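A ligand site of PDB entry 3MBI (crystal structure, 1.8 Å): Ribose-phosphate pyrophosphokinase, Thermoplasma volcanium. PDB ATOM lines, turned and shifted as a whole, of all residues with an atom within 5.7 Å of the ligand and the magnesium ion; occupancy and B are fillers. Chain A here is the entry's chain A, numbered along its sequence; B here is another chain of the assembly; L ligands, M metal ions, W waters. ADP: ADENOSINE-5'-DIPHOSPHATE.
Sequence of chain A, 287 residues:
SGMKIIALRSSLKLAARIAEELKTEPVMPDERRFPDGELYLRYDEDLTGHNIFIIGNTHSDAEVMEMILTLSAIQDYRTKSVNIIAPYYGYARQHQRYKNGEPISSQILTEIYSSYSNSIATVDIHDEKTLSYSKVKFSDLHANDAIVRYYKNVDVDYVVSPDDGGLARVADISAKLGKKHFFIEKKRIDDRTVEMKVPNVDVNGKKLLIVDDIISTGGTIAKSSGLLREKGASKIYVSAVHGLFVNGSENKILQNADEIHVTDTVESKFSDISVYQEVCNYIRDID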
ATOM      1  N   ARG A  93      15.439  -3.470   4.243  1.00  0.00           N
ATOM      2  CA  ARG A  93      15.458  -3.309   2.800  1.00  0.00           C
ATOM      3  C   ARG A  93      16.655  -4.028   2.176  1.00  0.00           C
ATOM      4  O   ARG A  93      16.705  -4.212   0.967  1.00  0.00           O
ATOM      5  CB  ARG A  93      15.429  -1.820   2.405  1.00  0.00           C
ATOM      6  CG  ARG A  93      14.140  -1.131   2.912  1.00  0.00           C
ATOM      7  CD  ARG A  93      14.192   0.385   2.783  1.00  0.00           C
ATOM      8  NE  ARG A  93      14.290   0.780   1.381  1.00  0.00           N
ATOM      9  CZ  ARG A  93      13.915   1.964   0.903  1.00  0.00           C
ATOM     10  NH1 ARG A  93      13.457   2.896   1.719  1.00  0.00           N
ATOM     11  NH2 ARG A  93      14.006   2.216  -0.397  1.00  0.00           N
ATOM     12  N   GLN A  94      17.630  -4.411   2.999  1.00  0.00           N
ATOM     13  CA  GLN A  94      18.770  -5.197   2.488  1.00  0.00           C
ATOM     14  C   GLN A  94      18.652  -6.612   3.037  1.00  0.00           C
ATOM     15  O   GLN A  94      19.449  -7.052   3.886  1.00  0.00           O
ATOM     16  CB  GLN A  94      20.110  -4.558   2.884  1.00  0.00           C
ATOM     17  CG  GLN A  94      21.359  -5.199   2.234  1.00  0.00           C
ATOM     18  CD  GLN A  94      21.455  -4.941   0.733  1.00  0.00           C
ATOM     19  OE1 GLN A  94      20.688  -4.162   0.175  1.00  0.00           O
ATOM     20  NE2 GLN A  94      22.370  -5.642   0.072  1.00  0.00           N
ATOM     21  N   HIS A  95      17.644  -7.319   2.538  1.00  0.00           N
ATOM     22  CA  HIS A  95      17.299  -8.660   3.010  1.00  0.00           C
ATOM     23  C   HIS A  95      17.848  -9.770   2.120  1.00  0.00           C
ATOM     24  O   HIS A  95      17.552 -10.938   2.346  1.00  0.00           O
ATOM     25  CB  HIS A  95      15.773  -8.788   3.122  1.00  0.00           C
ATOM     26  CG  HIS A  95      15.039  -8.353   1.885  1.00  0.00           C
ATOM     27  ND1 HIS A  95      14.861  -9.174   0.802  1.00  0.00           N
ATOM     28  CD2 HIS A  95      14.452  -7.175   1.575  1.00  0.00           C
ATOM     29  CE1 HIS A  95      14.186  -8.519  -0.137  1.00  0.00           C
ATOM     30  NE2 HIS A  95      13.921  -7.312   0.315  1.00  0.00           N
ATOM     31  N   TYR A  98      21.917  -8.121  -3.843  1.00  0.00           N
ATOM     32  CA  TYR A  98      21.434  -7.672  -5.146  1.00  0.00           C
ATOM     33  C   TYR A  98      22.581  -7.631  -6.159  1.00  0.00           C
ATOM     34  O   TYR A  98      22.357  -7.606  -7.372  1.00  0.00           O
ATOM     35  CB  TYR A  98      20.791  -6.304  -5.004  1.00  0.00           C
ATOM     36  CG  TYR A  98      19.551  -6.351  -4.152  1.00  0.00           C
ATOM     37  CD1 TYR A  98      18.300  -6.568  -4.720  1.00  0.00           C
ATOM     38  CD2 TYR A  98      19.628  -6.228  -2.779  1.00  0.00           C
ATOM     39  CE1 TYR A  98      17.163  -6.624  -3.919  1.00  0.00           C
ATOM     40  CE2 TYR A  98      18.514  -6.291  -1.982  1.00  0.00           C
ATOM     41  CZ  TYR A  98      17.281  -6.485  -2.560  1.00  0.00           C
ATOM     42  OH  TYR A  98      16.173  -6.544  -1.742  1.00  0.00           O
ATOM     43  N   GLU A 102      27.841  -7.958  -1.751  1.00  0.00           N
ATOM     44  CA  GLU A 102      27.053  -7.130  -0.826  1.00  0.00           C
ATOM     45  C   GLU A 102      26.781  -7.895   0.467  1.00  0.00           C
ATOM     46  O   GLU A 102      26.721  -9.134   0.457  1.00  0.00           O
ATOM     47  CB  GLU A 102      25.691  -6.749  -1.449  1.00  0.00           C
ATOM     48  CG  GLU A 102      25.740  -5.725  -2.570  1.00  0.00           C
ATOM     49  CD  GLU A 102      24.360  -5.385  -3.096  1.00  0.00           C
ATOM     50  OE1 GLU A 102      23.369  -5.993  -2.657  1.00  0.00           O
ATOM     51  OE2 GLU A 102      24.264  -4.486  -3.953  1.00  0.00           O
ATOM     52  N   HIS A 126       9.683  -4.774   6.298  1.00  0.00           N
ATOM     53  CA  HIS A 126       9.638  -4.500   4.867  1.00  0.00           C
ATOM     54  C   HIS A 126       9.482  -5.777   4.029  1.00  0.00           C
ATOM     55  O   HIS A 126       8.790  -5.778   3.016  1.00  0.00           O
ATOM     56  CB  HIS A 126      10.890  -3.737   4.410  1.00  0.00           C
ATOM     57  CG  HIS A 126      10.853  -3.349   2.980  1.00  0.00           C
ATOM     58  ND1 HIS A 126       9.842  -2.570   2.437  1.00  0.00           N
ATOM     59  CD2 HIS A 126      11.681  -3.652   1.940  1.00  0.00           C
ATOM     60  CE1 HIS A 126      10.054  -2.398   1.146  1.00  0.00           C
ATOM     61  NE2 HIS A 126      11.164  -3.044   0.816  1.00  0.00           N
ATOM     62  N   ASP A 127      10.161  -6.845   4.446  1.00  0.00           N
ATOM     63  CA  ASP A 127      10.093  -8.111   3.733  1.00  0.00           C
ATOM     64  C   ASP A 127      10.195  -9.270   4.714  1.00  0.00           C
ATOM     65  O   ASP A 127      11.110  -9.315   5.537  1.00  0.00           O
ATOM     66  CB  ASP A 127      11.184  -8.190   2.652  1.00  0.00           C
ATOM     67  CG  ASP A 127      10.975  -9.348   1.692  1.00  0.00           C
ATOM     68  OD1 ASP A 127      10.806  -9.100   0.478  1.00  0.00           O
ATOM     69  OD2 ASP A 127      10.994 -10.506   2.140  1.00  0.00           O
ATOM     70  N   ASP A 163       2.678  -0.559  -4.348  1.00  0.00           N
ATOM     71  CA  ASP A 163       3.423  -1.708  -4.839  1.00  0.00           C
ATOM     72  C   ASP A 163       2.638  -2.992  -4.618  1.00  0.00           C
ATOM     73  O   ASP A 163       1.602  -2.987  -3.954  1.00  0.00           O
ATOM     74  CB  ASP A 163       4.824  -1.784  -4.200  1.00  0.00           C
ATOM     75  CG  ASP A 163       4.779  -2.012  -2.686  1.00  0.00           C
ATOM     76  OD1 ASP A 163       3.707  -2.344  -2.141  1.00  0.00           O
ATOM     77  OD2 ASP A 163       5.831  -1.861  -2.042  1.00  0.00           O
ATOM     78  N   LYS A 186       5.272  -1.453  -8.969  1.00  0.00           N
ATOM     79  CA  LYS A 186       6.393  -0.571  -8.705  1.00  0.00           C
ATOM     80  C   LYS A 186       7.710  -1.246  -9.063  1.00  0.00           C
ATOM     81  O   LYS A 186       7.878  -2.435  -8.824  1.00  0.00           O
ATOM     82  CB  LYS A 186       6.397  -0.172  -7.232  1.00  0.00           C
ATOM     83  CG  LYS A 186       7.559   0.734  -6.834  1.00  0.00           C
ATOM     84  CD  LYS A 186       7.573   0.946  -5.318  1.00  0.00           C
ATOM     85  CE  LYS A 186       8.964   1.151  -4.790  1.00  0.00           C
ATOM     86  NZ  LYS A 186       8.979   1.156  -3.300  1.00  0.00           N
ATOM     87  N   ARG A 188      11.805  -0.188  -8.405  1.00  0.00           N
ATOM     88  CA  ARG A 188      12.772   0.790  -7.889  1.00  0.00           C
ATOM     89  C   ARG A 188      13.997   0.898  -8.813  1.00  0.00           C
ATOM     90  O   ARG A 188      14.596  -0.100  -9.201  1.00  0.00           O
ATOM     91  CB  ARG A 188      13.177   0.467  -6.455  1.00  0.00           C
ATOM     92  CG  ARG A 188      14.336   1.335  -5.945  1.00  0.00           C
ATOM     93  CD  ARG A 188      14.543   1.190  -4.448  1.00  0.00           C
ATOM     94  NE  ARG A 188      13.402   1.603  -3.651  1.00  0.00           N
ATOM     95  CZ  ARG A 188      12.995   2.858  -3.512  1.00  0.00           C
ATOM     96  NH1 ARG A 188      13.647   3.835  -4.132  1.00  0.00           N
ATOM     97  NH2 ARG A 188      11.941   3.150  -2.746  1.00  0.00           N
ATOM     98  N   ASP A 191      18.155   4.752  -5.260  1.00  0.00           N
ATOM     99  CA  ASP A 191      17.786   5.165  -3.895  1.00  0.00           C
ATOM    100  C   ASP A 191      16.642   6.178  -3.859  1.00  0.00           C
ATOM    101  O   ASP A 191      15.925   6.311  -2.858  1.00  0.00           O
ATOM    102  CB  ASP A 191      18.985   5.808  -3.193  1.00  0.00           C
ATOM    103  CG  ASP A 191      20.113   4.830  -2.934  1.00  0.00           C
ATOM    104  OD1 ASP A 191      20.039   3.675  -3.396  1.00  0.00           O
ATOM    105  OD2 ASP A 191      21.095   5.254  -2.290  1.00  0.00           O
ATOM    106  N   SER A 216      10.770   7.181   3.077  1.00  0.00           N
ATOM    107  CA  SER A 216      12.156   7.591   3.288  1.00  0.00           C
ATOM    108  C   SER A 216      12.395   8.897   2.523  1.00  0.00           C
ATOM    109  O   SER A 216      12.162   9.987   3.061  1.00  0.00           O
ATOM    110  CB  SER A 216      13.127   6.490   2.868  1.00  0.00           C
ATOM    111  OG  SER A 216      14.479   6.781   3.241  1.00  0.00           O
ATOM    112  N   ARG B  32      28.694   3.516   0.667  1.00  0.00           N
ATOM    113  CA  ARG B  32      27.870   4.720   0.648  1.00  0.00           C
ATOM    114  C   ARG B  32      26.805   4.650   1.733  1.00  0.00           C
ATOM    115  O   ARG B  32      26.587   3.583   2.329  1.00  0.00           O
ATOM    116  CB  ARG B  32      27.210   4.925  -0.730  1.00  0.00           C
ATOM    117  CG  ARG B  32      25.961   4.080  -1.012  1.00  0.00           C
ATOM    118  CD  ARG B  32      25.212   4.635  -2.242  1.00  0.00           C
ATOM    119  NE  ARG B  32      23.948   3.958  -2.544  1.00  0.00           N
ATOM    120  CZ  ARG B  32      23.872   2.751  -3.100  1.00  0.00           C
ATOM    121  NH1 ARG B  32      24.978   2.078  -3.391  1.00  0.00           N
ATOM    122  NH2 ARG B  32      22.691   2.207  -3.364  1.00  0.00           N
ATOM    123  N   PHE B  34      22.804   5.044   2.416  1.00  0.00           N
ATOM    124  CA  PHE B  34      21.461   5.222   1.861  1.00  0.00           C
ATOM    125  C   PHE B  34      20.871   6.554   2.367  1.00  0.00           C
ATOM    126  O   PHE B  34      21.344   7.107   3.354  1.00  0.00           O
ATOM    127  CB  PHE B  34      20.573   4.042   2.242  1.00  0.00           C
ATOM    128  CG  PHE B  34      20.881   2.773   1.479  1.00  0.00           C
ATOM    129  CD1 PHE B  34      20.615   2.700   0.112  1.00  0.00           C
ATOM    130  CD2 PHE B  34      21.429   1.670   2.120  1.00  0.00           C
ATOM    131  CE1 PHE B  34      20.895   1.534  -0.601  1.00  0.00           C
ATOM    132  CE2 PHE B  34      21.696   0.503   1.407  1.00  0.00           C
ATOM    133  CZ  PHE B  34      21.435   0.441   0.046  1.00  0.00           C
ATOM    134  N   PRO B  35      19.824   7.067   1.710  1.00  0.00           N
ATOM    135  CA  PRO B  35      19.259   8.344   2.153  1.00  0.00           C
ATOM    136  C   PRO B  35      18.791   8.364   3.622  1.00  0.00           C
ATOM    137  O   PRO B  35      18.796   9.442   4.225  1.00  0.00           O
ATOM    138  CB  PRO B  35      18.057   8.530   1.219  1.00  0.00           C
ATOM    139  CG  PRO B  35      18.464   7.799  -0.036  1.00  0.00           C
ATOM    140  CD  PRO B  35      19.223   6.592   0.457  1.00  0.00           C
ATOM    141  N   ASP B  36      18.402   7.219   4.162  1.00  0.00           N
ATOM    142  CA  ASP B  36      17.952   7.110   5.555  1.00  0.00           C
ATOM    143  C   ASP B  36      19.110   6.882   6.541  1.00  0.00           C
ATOM    144  O   ASP B  36      18.898   6.604   7.723  1.00  0.00           O
ATOM    145  CB  ASP B  36      16.935   5.970   5.697  1.00  0.00           C
ATOM    146  CG  ASP B  36      17.497   4.635   5.204  1.00  0.00           C
ATOM    147  OD1 ASP B  36      18.717   4.571   4.955  1.00  0.00           O
ATOM    148  OD2 ASP B  36      16.719   3.664   5.054  1.00  0.00           O
ATOM    149  N   GLU B  38      21.383   4.449   6.501  1.00  0.00           N
ATOM    150  CA  GLU B  38      21.882   3.075   6.601  1.00  0.00           C
ATOM    151  C   GLU B  38      23.135   2.890   5.748  1.00  0.00           C
ATOM    152  O   GLU B  38      23.299   3.535   4.712  1.00  0.00           O
ATOM    153  CB  GLU B  38      20.789   2.060   6.211  1.00  0.00           C
ATOM    154  CG  GLU B  38      19.662   1.983   7.243  1.00  0.00           C
ATOM    155  CD  GLU B  38      18.678   0.851   6.994  1.00  0.00           C
ATOM    156  OE1 GLU B  38      18.845   0.085   6.037  1.00  0.00           O
ATOM    157  OE2 GLU B  38      17.736   0.707   7.809  1.00  0.00           O
ATOM    158  N   TYR B  40      25.740   1.105   3.234  1.00  0.00           N
ATOM    159  CA  TYR B  40      25.866   0.151   2.132  1.00  0.00           C
ATOM    160  C   TYR B  40      27.336  -0.102   1.833  1.00  0.00           C
ATOM    161  O   TYR B  40      28.133   0.839   1.795  1.00  0.00           O
ATOM    162  CB  TYR B  40      25.199   0.696   0.872  1.00  0.00           C
ATOM    163  CG  TYR B  40      25.441  -0.153  -0.364  1.00  0.00           C
ATOM    164  CD1 TYR B  40      24.518  -1.119  -0.758  1.00  0.00           C
ATOM    165  CD2 TYR B  40      26.605  -0.016  -1.131  1.00  0.00           C
ATOM    166  CE1 TYR B  40      24.722  -1.899  -1.883  1.00  0.00           C
ATOM    167  CE2 TYR B  40      26.817  -0.797  -2.277  1.00  0.00           C
ATOM    168  CZ  TYR B  40      25.861  -1.744  -2.632  1.00  0.00           C
ATOM    169  OH  TYR B  40      26.031  -2.537  -3.735  1.00  0.00           O
HETATM  170  PB  ADP L   1      11.597  -1.849  -2.664  1.00  0.00           P
HETATM  171  O1B ADP L   1      12.175  -0.510  -2.325  1.00  0.00           O
HETATM  172  O2B ADP L   1      11.964  -2.990  -1.750  1.00  0.00           O
HETATM  173  O3B ADP L   1      10.155  -1.825  -3.085  1.00  0.00           O
HETATM  174  PA  ADP L   1      13.556  -3.242  -4.259  1.00  0.00           P
HETATM  175  O1A ADP L   1      13.850  -3.293  -5.727  1.00  0.00           O
HETATM  176  O2A ADP L   1      13.183  -4.515  -3.533  1.00  0.00           O
HETATM  177  O3A ADP L   1      12.369  -2.176  -4.060  1.00  0.00           O
HETATM  178  O5' ADP L   1      14.823  -2.529  -3.583  1.00  0.00           O
HETATM  179  C5' ADP L   1      16.048  -3.249  -3.513  1.00  0.00           C
HETATM  180  C4' ADP L   1      17.175  -2.222  -3.572  1.00  0.00           C
HETATM  181  O4' ADP L   1      17.083  -1.388  -2.412  1.00  0.00           O
HETATM  182  C3' ADP L   1      18.520  -2.931  -3.504  1.00  0.00           C
HETATM  183  O3' ADP L   1      19.404  -2.347  -4.473  1.00  0.00           O
HETATM  184  C2' ADP L   1      19.027  -2.639  -2.114  1.00  0.00           C
HETATM  185  O2' ADP L   1      20.458  -2.584  -2.023  1.00  0.00           O
HETATM  186  C1' ADP L   1      18.385  -1.297  -1.854  1.00  0.00           C
HETATM  187  N9  ADP L   1      18.363  -0.909  -0.439  1.00  0.00           N
HETATM  188  C8  ADP L   1      18.761  -1.640   0.608  1.00  0.00           C
HETATM  189  N7  ADP L   1      18.619  -0.929   1.751  1.00  0.00           N
HETATM  190  C5  ADP L   1      18.140   0.288   1.428  1.00  0.00           C
HETATM  191  C6  ADP L   1      17.762   1.518   2.143  1.00  0.00           C
HETATM  192  N6  ADP L   1      17.867   1.612   3.485  1.00  0.00           N
HETATM  193  N1  ADP L   1      17.300   2.553   1.414  1.00  0.00           N
HETATM  194  C2  ADP L   1      17.176   2.488   0.082  1.00  0.00           C
HETATM  195  N3  ADP L   1      17.493   1.401  -0.631  1.00  0.00           N
HETATM  196  C4  ADP L   1      17.971   0.292  -0.021  1.00  0.00           C
HETATM  197 MG    MG M   1      12.624  -5.258  -1.502  1.00  0.00          MG
HETATM  198  O   HOH W   1      11.878  -2.855  -7.344  1.00  0.00           O
HETATM  199  O   HOH W   2      16.288   5.213   1.680  1.00  0.00           O
HETATM  200  O   HOH W   3      13.499  -6.483  -6.468  1.00  0.00           O
HETATM  201  O   HOH W   4      14.082  -4.133  -0.329  1.00  0.00           O
HETATM  202  O   HOH W   5      11.145  -6.443  -0.581  1.00  0.00           O
HETATM  203  O   HOH W   6      20.277  -1.269   4.095  1.00  0.00           O
HETATM  204  O   HOH W   7      13.750  -6.592  -2.771  1.00  0.00           O
HETATM  205  O   HOH W   8      14.757  -0.767  -1.010  1.00  0.00           O
HETATM  206  O   HOH W   9      22.270  -2.922  -4.625  1.00  0.00           O
HETATM  207  O   HOH W  10      10.675  -5.416  -4.560  1.00  0.00           O
HETATM  208  O   HOH W  11      18.426  -3.288  -7.046  1.00  0.00           O
HETATM  209  O   HOH W  12      17.927   1.755  -3.557  1.00  0.00           O
HETATM  210  O   HOH W  13      10.623  -4.883  -2.108  1.00  0.00           O
HETATM  211  O   HOH W  14      10.889   0.994  -0.614  1.00  0.00           O
HETATM  212  O   HOH W  15       9.950  -2.076  -5.797  1.00  0.00           O
HETATM  213  O   HOH W  16      17.988   0.434  -5.946  1.00  0.00           O
HETATM  214  O   HOH W  17      16.051  -1.959  -7.112  1.00  0.00           O
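O2B of the ligand lies close to NE2 of His 126. OE1 of Gln 94 sits at hydrogen-bond distance from O2' of the ligand, at 2.7 Å. O1B of the ligand is in salt-bridge range of NE of Arg 188 (2.8 Å). The side-chain carboxylate (OD2) of Asp 36 of chain B is in hydrogen-bond range of a nitrogen (N6) of the ligand (2.8 Å). The side-chain carboxylate (OE1) of Glu 38 of chain B sits at hydrogen-bond distance from a nitrogen (N6) of the ligand. O3B of the ligand is in salt-bridge range of NZ of Lys 186 (3.2 Å). O1B of the ligand is in salt-bridge range of NH2 of Arg 93 (3.8 Å).
Water W13 lies within hydrogen-bond range of an oxygen (O3B) of the ligand (3.2 Å) and a ring nitrogen (NE2) of His 126 (3.5 Å). Water W4 lies within hydrogen-bond range of the backbone carbonyl oxygen (O) of Arg 93 (2.9 Å), a ring nitrogen (NE2) of His 95 (3.2 Å), a ring nitrogen (NE2) of His 126 (3.3 Å) and the side-chain hydroxyl (OH) of Tyr 98 (3.5 Å). Water W1 bridges an oxygen (O1A) of the ligand (2.6 Å) and the backbone NH of Arg 188 (2.9 Å). Water W2 bridges N1 of the ligand (2.9 Å) and OG of Ser 216 (2.9 Å). Water W17 bridges O1A of the ligand and O of Arg 188. Water W12 bridges the side-chain carboxylate of Asp 191 and a nitrogen (N3) of the ligand.
Residues that only touch the magnesium ion: His 95, His 126 and Tyr 98. Along chain A the residues within 4 Å of the magnesium ion span positions 95 to 126. The nearest printed residue that does not touch the magnesium ion is Asp 127 (4.7 Å).
NE2 of Gln 94 lies within hydrogen-bond range of OE1 of Glu 102 (2.9 Å). The backbone NH (N) of Glu 38 of chain B sits at hydrogen-bond distance from the side-chain carboxylate (OD1) of Asp 36 of chain B (3.1 Å). NE2 of His 95 sits at hydrogen-bond distance from OH of Tyr 98 (3.1 Å). The side-chain carboxylate (OE1) of Glu 102 sits at hydrogen-bond distance from the backbone NH (N) of Tyr 98, 2.8 Å away.
CD2 of Tyr 98 touches C3' of the ligand, at 3.6 Å. CE1 of Phe 34 of chain B touches C4 of the ligand, at 3.2 Å. Hydrophobic or aromatic side chains within 4 Å of the ligand: Tyr 98, His 126 and Phe 34 of chain B. Within 4 Å of the ligand: Arg 93, Gln 94, Tyr 98, His 126, Lys 186, Arg 188, Phe 34 of chain B, Asp 36 of chain B and Glu 38 of chain B.
The magnesium ion is bound by water W5 (2.1 Å). The magnesium ion is bound by water W13 (2.1 Å). Water W7 is bound to the magnesium ion. Water W4 binds the magnesium ion, 2.2 Å away. O2A of the ligand binds the magnesium ion (2.2 Å). An oxygen (O2B) of the ligand is bound to the magnesium ion (2.4 Å). The magnesium ion has six donor atoms within binding distance.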
